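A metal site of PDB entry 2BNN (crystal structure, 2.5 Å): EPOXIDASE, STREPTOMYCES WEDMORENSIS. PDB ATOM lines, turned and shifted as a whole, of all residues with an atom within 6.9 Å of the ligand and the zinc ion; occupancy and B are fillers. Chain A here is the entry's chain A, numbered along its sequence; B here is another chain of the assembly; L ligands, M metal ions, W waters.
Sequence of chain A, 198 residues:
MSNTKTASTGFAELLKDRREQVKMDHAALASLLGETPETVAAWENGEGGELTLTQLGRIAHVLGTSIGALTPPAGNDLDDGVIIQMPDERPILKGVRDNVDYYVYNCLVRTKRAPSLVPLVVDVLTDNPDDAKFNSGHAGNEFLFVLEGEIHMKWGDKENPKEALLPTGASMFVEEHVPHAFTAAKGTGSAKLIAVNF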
ATOM      1  N   ARG A  97      -6.588   6.956 -15.649  1.00  0.00           N
ATOM      2  CA  ARG A  97      -6.750   5.840 -16.610  1.00  0.00           C
ATOM      3  C   ARG A  97      -8.212   5.451 -16.882  1.00  0.00           C
ATOM      4  O   ARG A  97      -8.605   5.317 -18.059  1.00  0.00           O
ATOM      5  CB  ARG A  97      -5.895   4.628 -16.219  1.00  0.00           C
ATOM      6  CG  ARG A  97      -4.408   4.992 -16.114  1.00  0.00           C
ATOM      7  CD  ARG A  97      -3.440   3.899 -16.543  1.00  0.00           C
ATOM      8  NE  ARG A  97      -2.162   4.487 -16.982  1.00  0.00           N
ATOM      9  CZ  ARG A  97      -1.059   3.780 -17.281  1.00  0.00           C
ATOM     10  NH1 ARG A  97      -1.049   2.455 -17.185  1.00  0.00           N
ATOM     11  NH2 ARG A  97       0.039   4.420 -17.677  1.00  0.00           N
ATOM     12  N   TYR A 103      -1.638   7.514 -11.264  1.00  0.00           N
ATOM     13  CA  TYR A 103      -0.263   7.951 -11.065  1.00  0.00           C
ATOM     14  C   TYR A 103      -0.176   9.466 -10.895  1.00  0.00           C
ATOM     15  O   TYR A 103      -1.038  10.200 -11.392  1.00  0.00           O
ATOM     16  CB  TYR A 103       0.598   7.578 -12.273  1.00  0.00           C
ATOM     17  CG  TYR A 103       0.772   6.106 -12.632  1.00  0.00           C
ATOM     18  CD1 TYR A 103       0.712   5.699 -13.963  1.00  0.00           C
ATOM     19  CD2 TYR A 103       1.037   5.147 -11.654  1.00  0.00           C
ATOM     20  CE1 TYR A 103       0.893   4.363 -14.325  1.00  0.00           C
ATOM     21  CE2 TYR A 103       1.211   3.791 -12.005  1.00  0.00           C
ATOM     22  CZ  TYR A 103       1.150   3.410 -13.349  1.00  0.00           C
ATOM     23  OH  TYR A 103       1.316   2.087 -13.714  1.00  0.00           O
ATOM     24  N   TYR A 105       2.868  11.946 -12.057  1.00  0.00           N
ATOM     25  CA  TYR A 105       4.164  12.080 -12.712  1.00  0.00           C
ATOM     26  C   TYR A 105       4.913  13.344 -12.287  1.00  0.00           C
ATOM     27  O   TYR A 105       4.458  14.458 -12.550  1.00  0.00           O
ATOM     28  CB  TYR A 105       3.978  12.118 -14.225  1.00  0.00           C
ATOM     29  CG  TYR A 105       3.271  10.918 -14.802  1.00  0.00           C
ATOM     30  CD1 TYR A 105       1.985  11.044 -15.328  1.00  0.00           C
ATOM     31  CD2 TYR A 105       3.879   9.670 -14.824  1.00  0.00           C
ATOM     32  CE1 TYR A 105       1.326   9.933 -15.863  1.00  0.00           C
ATOM     33  CE2 TYR A 105       3.232   8.561 -15.347  1.00  0.00           C
ATOM     34  CZ  TYR A 105       1.953   8.695 -15.872  1.00  0.00           C
ATOM     35  OH  TYR A 105       1.320   7.601 -16.404  1.00  0.00           O
ATOM     36  N   VAL A 118      13.386  10.349 -20.884  1.00  0.00           N
ATOM     37  CA  VAL A 118      12.249  10.865 -20.121  1.00  0.00           C
ATOM     38  C   VAL A 118      12.209  10.219 -18.733  1.00  0.00           C
ATOM     39  O   VAL A 118      11.561   9.162 -18.524  1.00  0.00           O
ATOM     40  CB  VAL A 118      10.892  10.661 -20.843  1.00  0.00           C
ATOM     41  CG1 VAL A 118       9.777  11.378 -20.086  1.00  0.00           C
ATOM     42  CG2 VAL A 118      10.941  11.135 -22.294  1.00  0.00           C
ATOM     43  N   LEU A 120      11.383  10.149 -14.556  1.00  0.00           N
ATOM     44  CA  LEU A 120      10.249  10.544 -13.729  1.00  0.00           C
ATOM     45  C   LEU A 120      10.336   9.925 -12.339  1.00  0.00           C
ATOM     46  O   LEU A 120      10.757   8.780 -12.193  1.00  0.00           O
ATOM     47  CB  LEU A 120       8.936  10.053 -14.320  1.00  0.00           C
ATOM     48  CG  LEU A 120       8.578  10.150 -15.801  1.00  0.00           C
ATOM     49  CD1 LEU A 120       7.679   8.979 -16.172  1.00  0.00           C
ATOM     50  CD2 LEU A 120       7.918  11.483 -16.105  1.00  0.00           C
ATOM     51  N   VAL A 122       7.517   8.651 -10.183  1.00  0.00           N
ATOM     52  CA  VAL A 122       6.113   8.300 -10.355  1.00  0.00           C
ATOM     53  C   VAL A 122       5.499   7.964  -8.986  1.00  0.00           C
ATOM     54  O   VAL A 122       5.896   7.005  -8.341  1.00  0.00           O
ATOM     55  CB  VAL A 122       5.992   7.113 -11.342  1.00  0.00           C
ATOM     56  CG1 VAL A 122       4.566   6.666 -11.530  1.00  0.00           C
ATOM     57  CG2 VAL A 122       6.636   7.462 -12.687  1.00  0.00           C
ATOM     58  N   LYS A 133      -3.921  -1.035 -13.902  1.00  0.00           N
ATOM     59  CA  LYS A 133      -4.312  -0.585 -15.220  1.00  0.00           C
ATOM     60  C   LYS A 133      -3.099  -0.525 -16.129  1.00  0.00           C
ATOM     61  O   LYS A 133      -2.158   0.234 -15.892  1.00  0.00           O
ATOM     62  CB  LYS A 133      -5.038   0.754 -15.128  1.00  0.00           C
ATOM     63  CG  LYS A 133      -6.266   0.828 -16.016  1.00  0.00           C
ATOM     64  CD  LYS A 133      -7.465   1.394 -15.260  1.00  0.00           C
ATOM     65  CE  LYS A 133      -8.158   0.339 -14.406  1.00  0.00           C
ATOM     66  NZ  LYS A 133      -9.105   0.961 -13.434  1.00  0.00           N
ATOM     67  N   PHE A 134      -3.142  -1.361 -17.167  1.00  0.00           N
ATOM     68  CA  PHE A 134      -2.061  -1.513 -18.131  1.00  0.00           C
ATOM     69  C   PHE A 134      -2.002  -0.351 -19.108  1.00  0.00           C
ATOM     70  O   PHE A 134      -3.042   0.175 -19.526  1.00  0.00           O
ATOM     71  CB  PHE A 134      -2.276  -2.788 -18.943  1.00  0.00           C
ATOM     72  CG  PHE A 134      -1.788  -4.028 -18.262  1.00  0.00           C
ATOM     73  CD1 PHE A 134      -2.524  -4.632 -17.247  1.00  0.00           C
ATOM     74  CD2 PHE A 134      -0.574  -4.600 -18.657  1.00  0.00           C
ATOM     75  CE1 PHE A 134      -2.057  -5.774 -16.632  1.00  0.00           C
ATOM     76  CE2 PHE A 134      -0.099  -5.762 -18.037  1.00  0.00           C
ATOM     77  CZ  PHE A 134      -0.844  -6.346 -17.026  1.00  0.00           C
ATOM     78  N   ASN A 135      -0.798   0.049 -19.501  1.00  0.00           N
ATOM     79  CA  ASN A 135      -0.655   0.809 -20.728  1.00  0.00           C
ATOM     80  C   ASN A 135      -0.628  -0.220 -21.876  1.00  0.00           C
ATOM     81  O   ASN A 135      -0.883  -1.402 -21.641  1.00  0.00           O
ATOM     82  CB  ASN A 135       0.598   1.700 -20.701  1.00  0.00           C
ATOM     83  CG  ASN A 135       1.870   0.951 -20.349  1.00  0.00           C
ATOM     84  OD1 ASN A 135       1.908  -0.289 -20.338  1.00  0.00           O
ATOM     85  ND2 ASN A 135       2.936   1.696 -20.077  1.00  0.00           N
ATOM     86  N   GLY A 137       2.111  -0.648 -23.680  1.00  0.00           N
ATOM     87  CA  GLY A 137       3.542  -0.552 -23.978  1.00  0.00           C
ATOM     88  C   GLY A 137       3.841   0.784 -24.630  1.00  0.00           C
ATOM     89  O   GLY A 137       2.945   1.408 -25.183  1.00  0.00           O
ATOM     90  N   HIS A 138       5.096   1.222 -24.566  1.00  0.00           N
ATOM     91  CA  HIS A 138       5.461   2.479 -25.218  1.00  0.00           C
ATOM     92  C   HIS A 138       6.794   2.420 -25.958  1.00  0.00           C
ATOM     93  O   HIS A 138       7.499   1.399 -25.893  1.00  0.00           O
ATOM     94  CB  HIS A 138       5.409   3.678 -24.245  1.00  0.00           C
ATOM     95  CG  HIS A 138       5.971   3.384 -22.889  1.00  0.00           C
ATOM     96  ND1 HIS A 138       7.258   2.940 -22.688  1.00  0.00           N
ATOM     97  CD2 HIS A 138       5.405   3.479 -21.657  1.00  0.00           C
ATOM     98  CE1 HIS A 138       7.463   2.771 -21.393  1.00  0.00           C
ATOM     99  NE2 HIS A 138       6.362   3.097 -20.748  1.00  0.00           N
ATOM    100  N   GLY A 140       9.889   3.854 -25.858  1.00  0.00           N
ATOM    101  CA  GLY A 140      11.237   3.728 -25.320  1.00  0.00           C
ATOM    102  C   GLY A 140      11.456   2.442 -24.522  1.00  0.00           C
ATOM    103  O   GLY A 140      10.504   1.809 -24.057  1.00  0.00           O
ATOM    104  N   GLU A 142      12.761   1.134 -20.914  1.00  0.00           N
ATOM    105  CA  GLU A 142      12.562   1.752 -19.603  1.00  0.00           C
ATOM    106  C   GLU A 142      13.314   1.096 -18.430  1.00  0.00           C
ATOM    107  O   GLU A 142      13.166  -0.109 -18.172  1.00  0.00           O
ATOM    108  CB  GLU A 142      11.070   1.859 -19.297  1.00  0.00           C
ATOM    109  CG  GLU A 142      10.733   2.911 -18.251  1.00  0.00           C
ATOM    110  CD  GLU A 142       9.275   3.293 -18.304  1.00  0.00           C
ATOM    111  OE1 GLU A 142       8.965   4.427 -18.746  1.00  0.00           O
ATOM    112  OE2 GLU A 142       8.442   2.453 -17.929  1.00  0.00           O
ATOM    113  N   LEU A 144      13.681   1.133 -14.280  1.00  0.00           N
ATOM    114  CA  LEU A 144      12.856   1.480 -13.133  1.00  0.00           C
ATOM    115  C   LEU A 144      13.479   1.050 -11.833  1.00  0.00           C
ATOM    116  O   LEU A 144      14.156   0.025 -11.773  1.00  0.00           O
ATOM    117  CB  LEU A 144      11.457   0.877 -13.217  1.00  0.00           C
ATOM    118  CG  LEU A 144      10.604   1.344 -14.391  1.00  0.00           C
ATOM    119  CD1 LEU A 144      10.424   0.180 -15.382  1.00  0.00           C
ATOM    120  CD2 LEU A 144       9.258   1.889 -13.887  1.00  0.00           C
ATOM    121  N   VAL A 174      12.152  -2.653 -18.568  1.00  0.00           N
ATOM    122  CA  VAL A 174      11.044  -2.998 -19.462  1.00  0.00           C
ATOM    123  C   VAL A 174      11.390  -2.608 -20.899  1.00  0.00           C
ATOM    124  O   VAL A 174      11.556  -1.428 -21.202  1.00  0.00           O
ATOM    125  CB  VAL A 174       9.695  -2.356 -19.040  1.00  0.00           C
ATOM    126  CG1 VAL A 174       8.593  -2.739 -20.021  1.00  0.00           C
ATOM    127  CG2 VAL A 174       9.298  -2.791 -17.649  1.00  0.00           C
ATOM    128  N   VAL A 178       6.559  -3.427 -24.620  1.00  0.00           N
ATOM    129  CA  VAL A 178       6.041  -4.372 -23.640  1.00  0.00           C
ATOM    130  C   VAL A 178       5.048  -3.673 -22.705  1.00  0.00           C
ATOM    131  O   VAL A 178       5.405  -2.683 -22.062  1.00  0.00           O
ATOM    132  CB  VAL A 178       7.167  -5.028 -22.815  1.00  0.00           C
ATOM    133  CG1 VAL A 178       6.581  -5.852 -21.656  1.00  0.00           C
ATOM    134  CG2 VAL A 178       8.046  -5.896 -23.693  1.00  0.00           C
ATOM    135  N   HIS A 180       2.745  -2.862 -19.475  1.00  0.00           N
ATOM    136  CA  HIS A 180       3.009  -3.009 -18.038  1.00  0.00           C
ATOM    137  C   HIS A 180       2.151  -2.108 -17.138  1.00  0.00           C
ATOM    138  O   HIS A 180       1.723  -1.022 -17.536  1.00  0.00           O
ATOM    139  CB  HIS A 180       4.488  -2.765 -17.737  1.00  0.00           C
ATOM    140  CG  HIS A 180       5.003  -1.478 -18.312  1.00  0.00           C
ATOM    141  ND1 HIS A 180       5.336  -1.342 -19.643  1.00  0.00           N
ATOM    142  CD2 HIS A 180       5.196  -0.262 -17.744  1.00  0.00           C
ATOM    143  CE1 HIS A 180       5.728  -0.103 -19.868  1.00  0.00           C
ATOM    144  NE2 HIS A 180       5.657   0.563 -18.732  1.00  0.00           N
ATOM    145  N   ALA A 181       1.918  -2.576 -15.917  1.00  0.00           N
ATOM    146  CA  ALA A 181       1.129  -1.851 -14.925  1.00  0.00           C
ATOM    147  C   ALA A 181       1.789  -1.942 -13.561  1.00  0.00           C
ATOM    148  O   ALA A 181       2.445  -2.924 -13.253  1.00  0.00           O
ATOM    149  CB  ALA A 181      -0.290  -2.406 -14.885  1.00  0.00           C
ATOM    150  N   PHE A 182       1.597  -0.917 -12.740  1.00  0.00           N
ATOM    151  CA  PHE A 182       2.103  -0.909 -11.385  1.00  0.00           C
ATOM    152  C   PHE A 182       1.010  -0.451 -10.424  1.00  0.00           C
ATOM    153  O   PHE A 182       0.219   0.436 -10.769  1.00  0.00           O
ATOM    154  CB  PHE A 182       3.267   0.074 -11.241  1.00  0.00           C
ATOM    155  CG  PHE A 182       4.383  -0.119 -12.214  1.00  0.00           C
ATOM    156  CD1 PHE A 182       4.520   0.728 -13.308  1.00  0.00           C
ATOM    157  CD2 PHE A 182       5.331  -1.138 -12.020  1.00  0.00           C
ATOM    158  CE1 PHE A 182       5.574   0.544 -14.222  1.00  0.00           C
ATOM    159  CE2 PHE A 182       6.389  -1.314 -12.925  1.00  0.00           C
ATOM    160  CZ  PHE A 182       6.509  -0.477 -14.031  1.00  0.00           C
ATOM    161  N   LEU A 193       8.184   5.208  -7.790  1.00  0.00           N
ATOM    162  CA  LEU A 193       9.130   4.704  -8.785  1.00  0.00           C
ATOM    163  C   LEU A 193      10.000   5.841  -9.276  1.00  0.00           C
ATOM    164  O   LEU A 193       9.534   6.969  -9.408  1.00  0.00           O
ATOM    165  CB  LEU A 193       8.393   4.114  -9.981  1.00  0.00           C
ATOM    166  CG  LEU A 193       7.597   2.829  -9.768  1.00  0.00           C
ATOM    167  CD1 LEU A 193       6.724   2.531 -10.991  1.00  0.00           C
ATOM    168  CD2 LEU A 193       8.522   1.643  -9.459  1.00  0.00           C
ATOM    169  N   ALA A 195      11.306   6.199 -12.847  1.00  0.00           N
ATOM    170  CA  ALA A 195      11.223   5.591 -14.163  1.00  0.00           C
ATOM    171  C   ALA A 195      12.122   6.393 -15.085  1.00  0.00           C
ATOM    172  O   ALA A 195      12.076   7.625 -15.086  1.00  0.00           O
ATOM    173  CB  ALA A 195       9.806   5.615 -14.663  1.00  0.00           C
ATOM    174  N   VAL A 196      12.957   5.684 -15.855  1.00  0.00           N
ATOM    175  CA  VAL A 196      13.798   6.343 -16.845  1.00  0.00           C
ATOM    176  C   VAL A 196      13.557   5.736 -18.211  1.00  0.00           C
ATOM    177  O   VAL A 196      14.006   4.618 -18.512  1.00  0.00           O
ATOM    178  CB  VAL A 196      15.271   6.293 -16.485  1.00  0.00           C
ATOM    179  CG1 VAL A 196      16.110   7.061 -17.528  1.00  0.00           C
ATOM    180  CG2 VAL A 196      15.518   6.842 -15.071  1.00  0.00           C
ATOM    181  N   ASN A 197      12.806   6.462 -19.033  1.00  0.00           N
ATOM    182  CA  ASN A 197      12.533   6.047 -20.384  1.00  0.00           C
ATOM    183  C   ASN A 197      13.679   6.581 -21.221  1.00  0.00           C
ATOM    184  O   ASN A 197      14.077   7.744 -21.069  1.00  0.00           O
ATOM    185  CB  ASN A 197      11.195   6.611 -20.853  1.00  0.00           C
ATOM    186  CG  ASN A 197      10.555   5.784 -21.956  1.00  0.00           C
ATOM    187  OD1 ASN A 197      10.393   6.257 -23.079  1.00  0.00           O
ATOM    188  ND2 ASN A 197      10.191   4.544 -21.643  1.00  0.00           N
ATOM    189  N   LYS B  23       4.401  12.984 -20.997  1.00  0.00           N
ATOM    190  CA  LYS B  23       3.339  13.066 -19.971  1.00  0.00           C
ATOM    191  C   LYS B  23       2.419  14.299 -20.018  1.00  0.00           C
ATOM    192  O   LYS B  23       1.646  14.513 -19.073  1.00  0.00           O
ATOM    193  CB  LYS B  23       3.904  12.909 -18.557  1.00  0.00           C
ATOM    194  CG  LYS B  23       4.625  11.619 -18.297  1.00  0.00           C
ATOM    195  CD  LYS B  23       3.762  10.415 -18.606  1.00  0.00           C
ATOM    196  CE  LYS B  23       4.639   9.254 -19.005  1.00  0.00           C
ATOM    197  NZ  LYS B  23       3.964   7.992 -18.638  1.00  0.00           N
HETATM  198  C1  LIG L   1       4.619   3.822 -15.917  1.00  0.00           C
HETATM  199  C2  LIG L   1       5.955   4.418 -15.486  1.00  0.00           C
HETATM  200  C3  LIG L   1       6.651   5.326 -16.509  1.00  0.00           C
HETATM  201  O1  LIG L   1       5.844   3.111 -16.049  1.00  0.00           O
HETATM  202  P1  LIG L   1       4.039   4.338 -17.555  1.00  0.00           P
HETATM  203  O2  LIG L   1       3.783   5.808 -17.386  1.00  0.00           O
HETATM  204  O3  LIG L   1       2.794   3.516 -17.792  1.00  0.00           O
HETATM  205  O4  LIG L   1       5.122   4.032 -18.554  1.00  0.00           O
HETATM  206 ZN    ZN M   1       6.532   2.489 -18.668  1.00  0.00          ZN
HETATM  207  O   HOH W   1       1.744   1.589 -16.652  1.00  0.00           O
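OE2 of Glu 142 binds the zinc ion, at 2.0 Å.
The zinc ion is bound by O4 of the ligand, 2.1 Å away.
The zinc ion is bound by NE2 of His 180.
The zinc ion is bound by NE2 of His 138, 2.2 Å away.
Slightly farther from the zinc ion lies O1 of the ligand (2.8 Å).
An oxygen (O2) of the ligand lies within salt-bridge range of the side-chain amino group (NZ) of Lys 23 of chain B, 2.5 Å away.
The guanidinium group of Arg 97 lies within salt-bridge range of an oxygen (O3) of the ligand (2.9 Å).
ND2 of Asn 135 lies within hydrogen-bond range of O3 of the ligand.
O2 of the ligand lies within hydrogen-bond range of OH of Tyr 105, 3.2 Å away.
Residues that only touch the zinc ion: Asn 135 (3.9 Å).
Of the 24 residues printed, 4 come within 4 Å of the zinc ion.
The side-chain amide nitrogen of Asn 197 sits at hydrogen-bond distance from the side-chain carboxylate of Glu 142 (3.1 Å).
O of Glu 142 sits at hydrogen-bond distance from N of Val 174.
The backbone NH (N) of His 180 sits at hydrogen-bond distance from the side-chain amide oxygen (OD1) of Asn 135, at 2.8 Å.
The backbone carbonyl oxygen (O) of Val 178 sits at hydrogen-bond distance from a ring nitrogen (ND1) of His 180 (2.8 Å).
The side-chain amino group (NZ) of Lys 23 of chain B sits close to the side-chain hydroxyl (OH) of Tyr 105 (3.5 Å).
The guanidinium group of Arg 97 is in hydrogen-bond range of the backbone carbonyl oxygen of Lys 133 (2.8 Å).
N of Gly 137 lies close to OD1 of Asn 135.
The backbone NH (N) of Phe 182 lies within hydrogen-bond range of the side-chain hydroxyl (OH) of Tyr 103 (3.2 Å).
Leu 120 touches the ligand.
CE1 of Phe 182 touches O1 of the ligand, 3.2 Å away.
Ala 195 touches the ligand.
Hydrophobic or aromatic side chains that line the ligand: Tyr 105, Leu 120, His 138, His 180, Phe 182 and Ala 195.
Of the 24 residues printed, 10 come within 4 Å of the ligand.
Water W1 lies within hydrogen-bond range of an oxygen (O3) of the ligand (2.5 Å), the backbone carbonyl oxygen (O) of His 180 (2.8 Å), the guanidinium group (NH1) of Arg 97 (3.0 Å) and the side-chain hydroxyl (OH) of Tyr 103 (3.0 Å).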
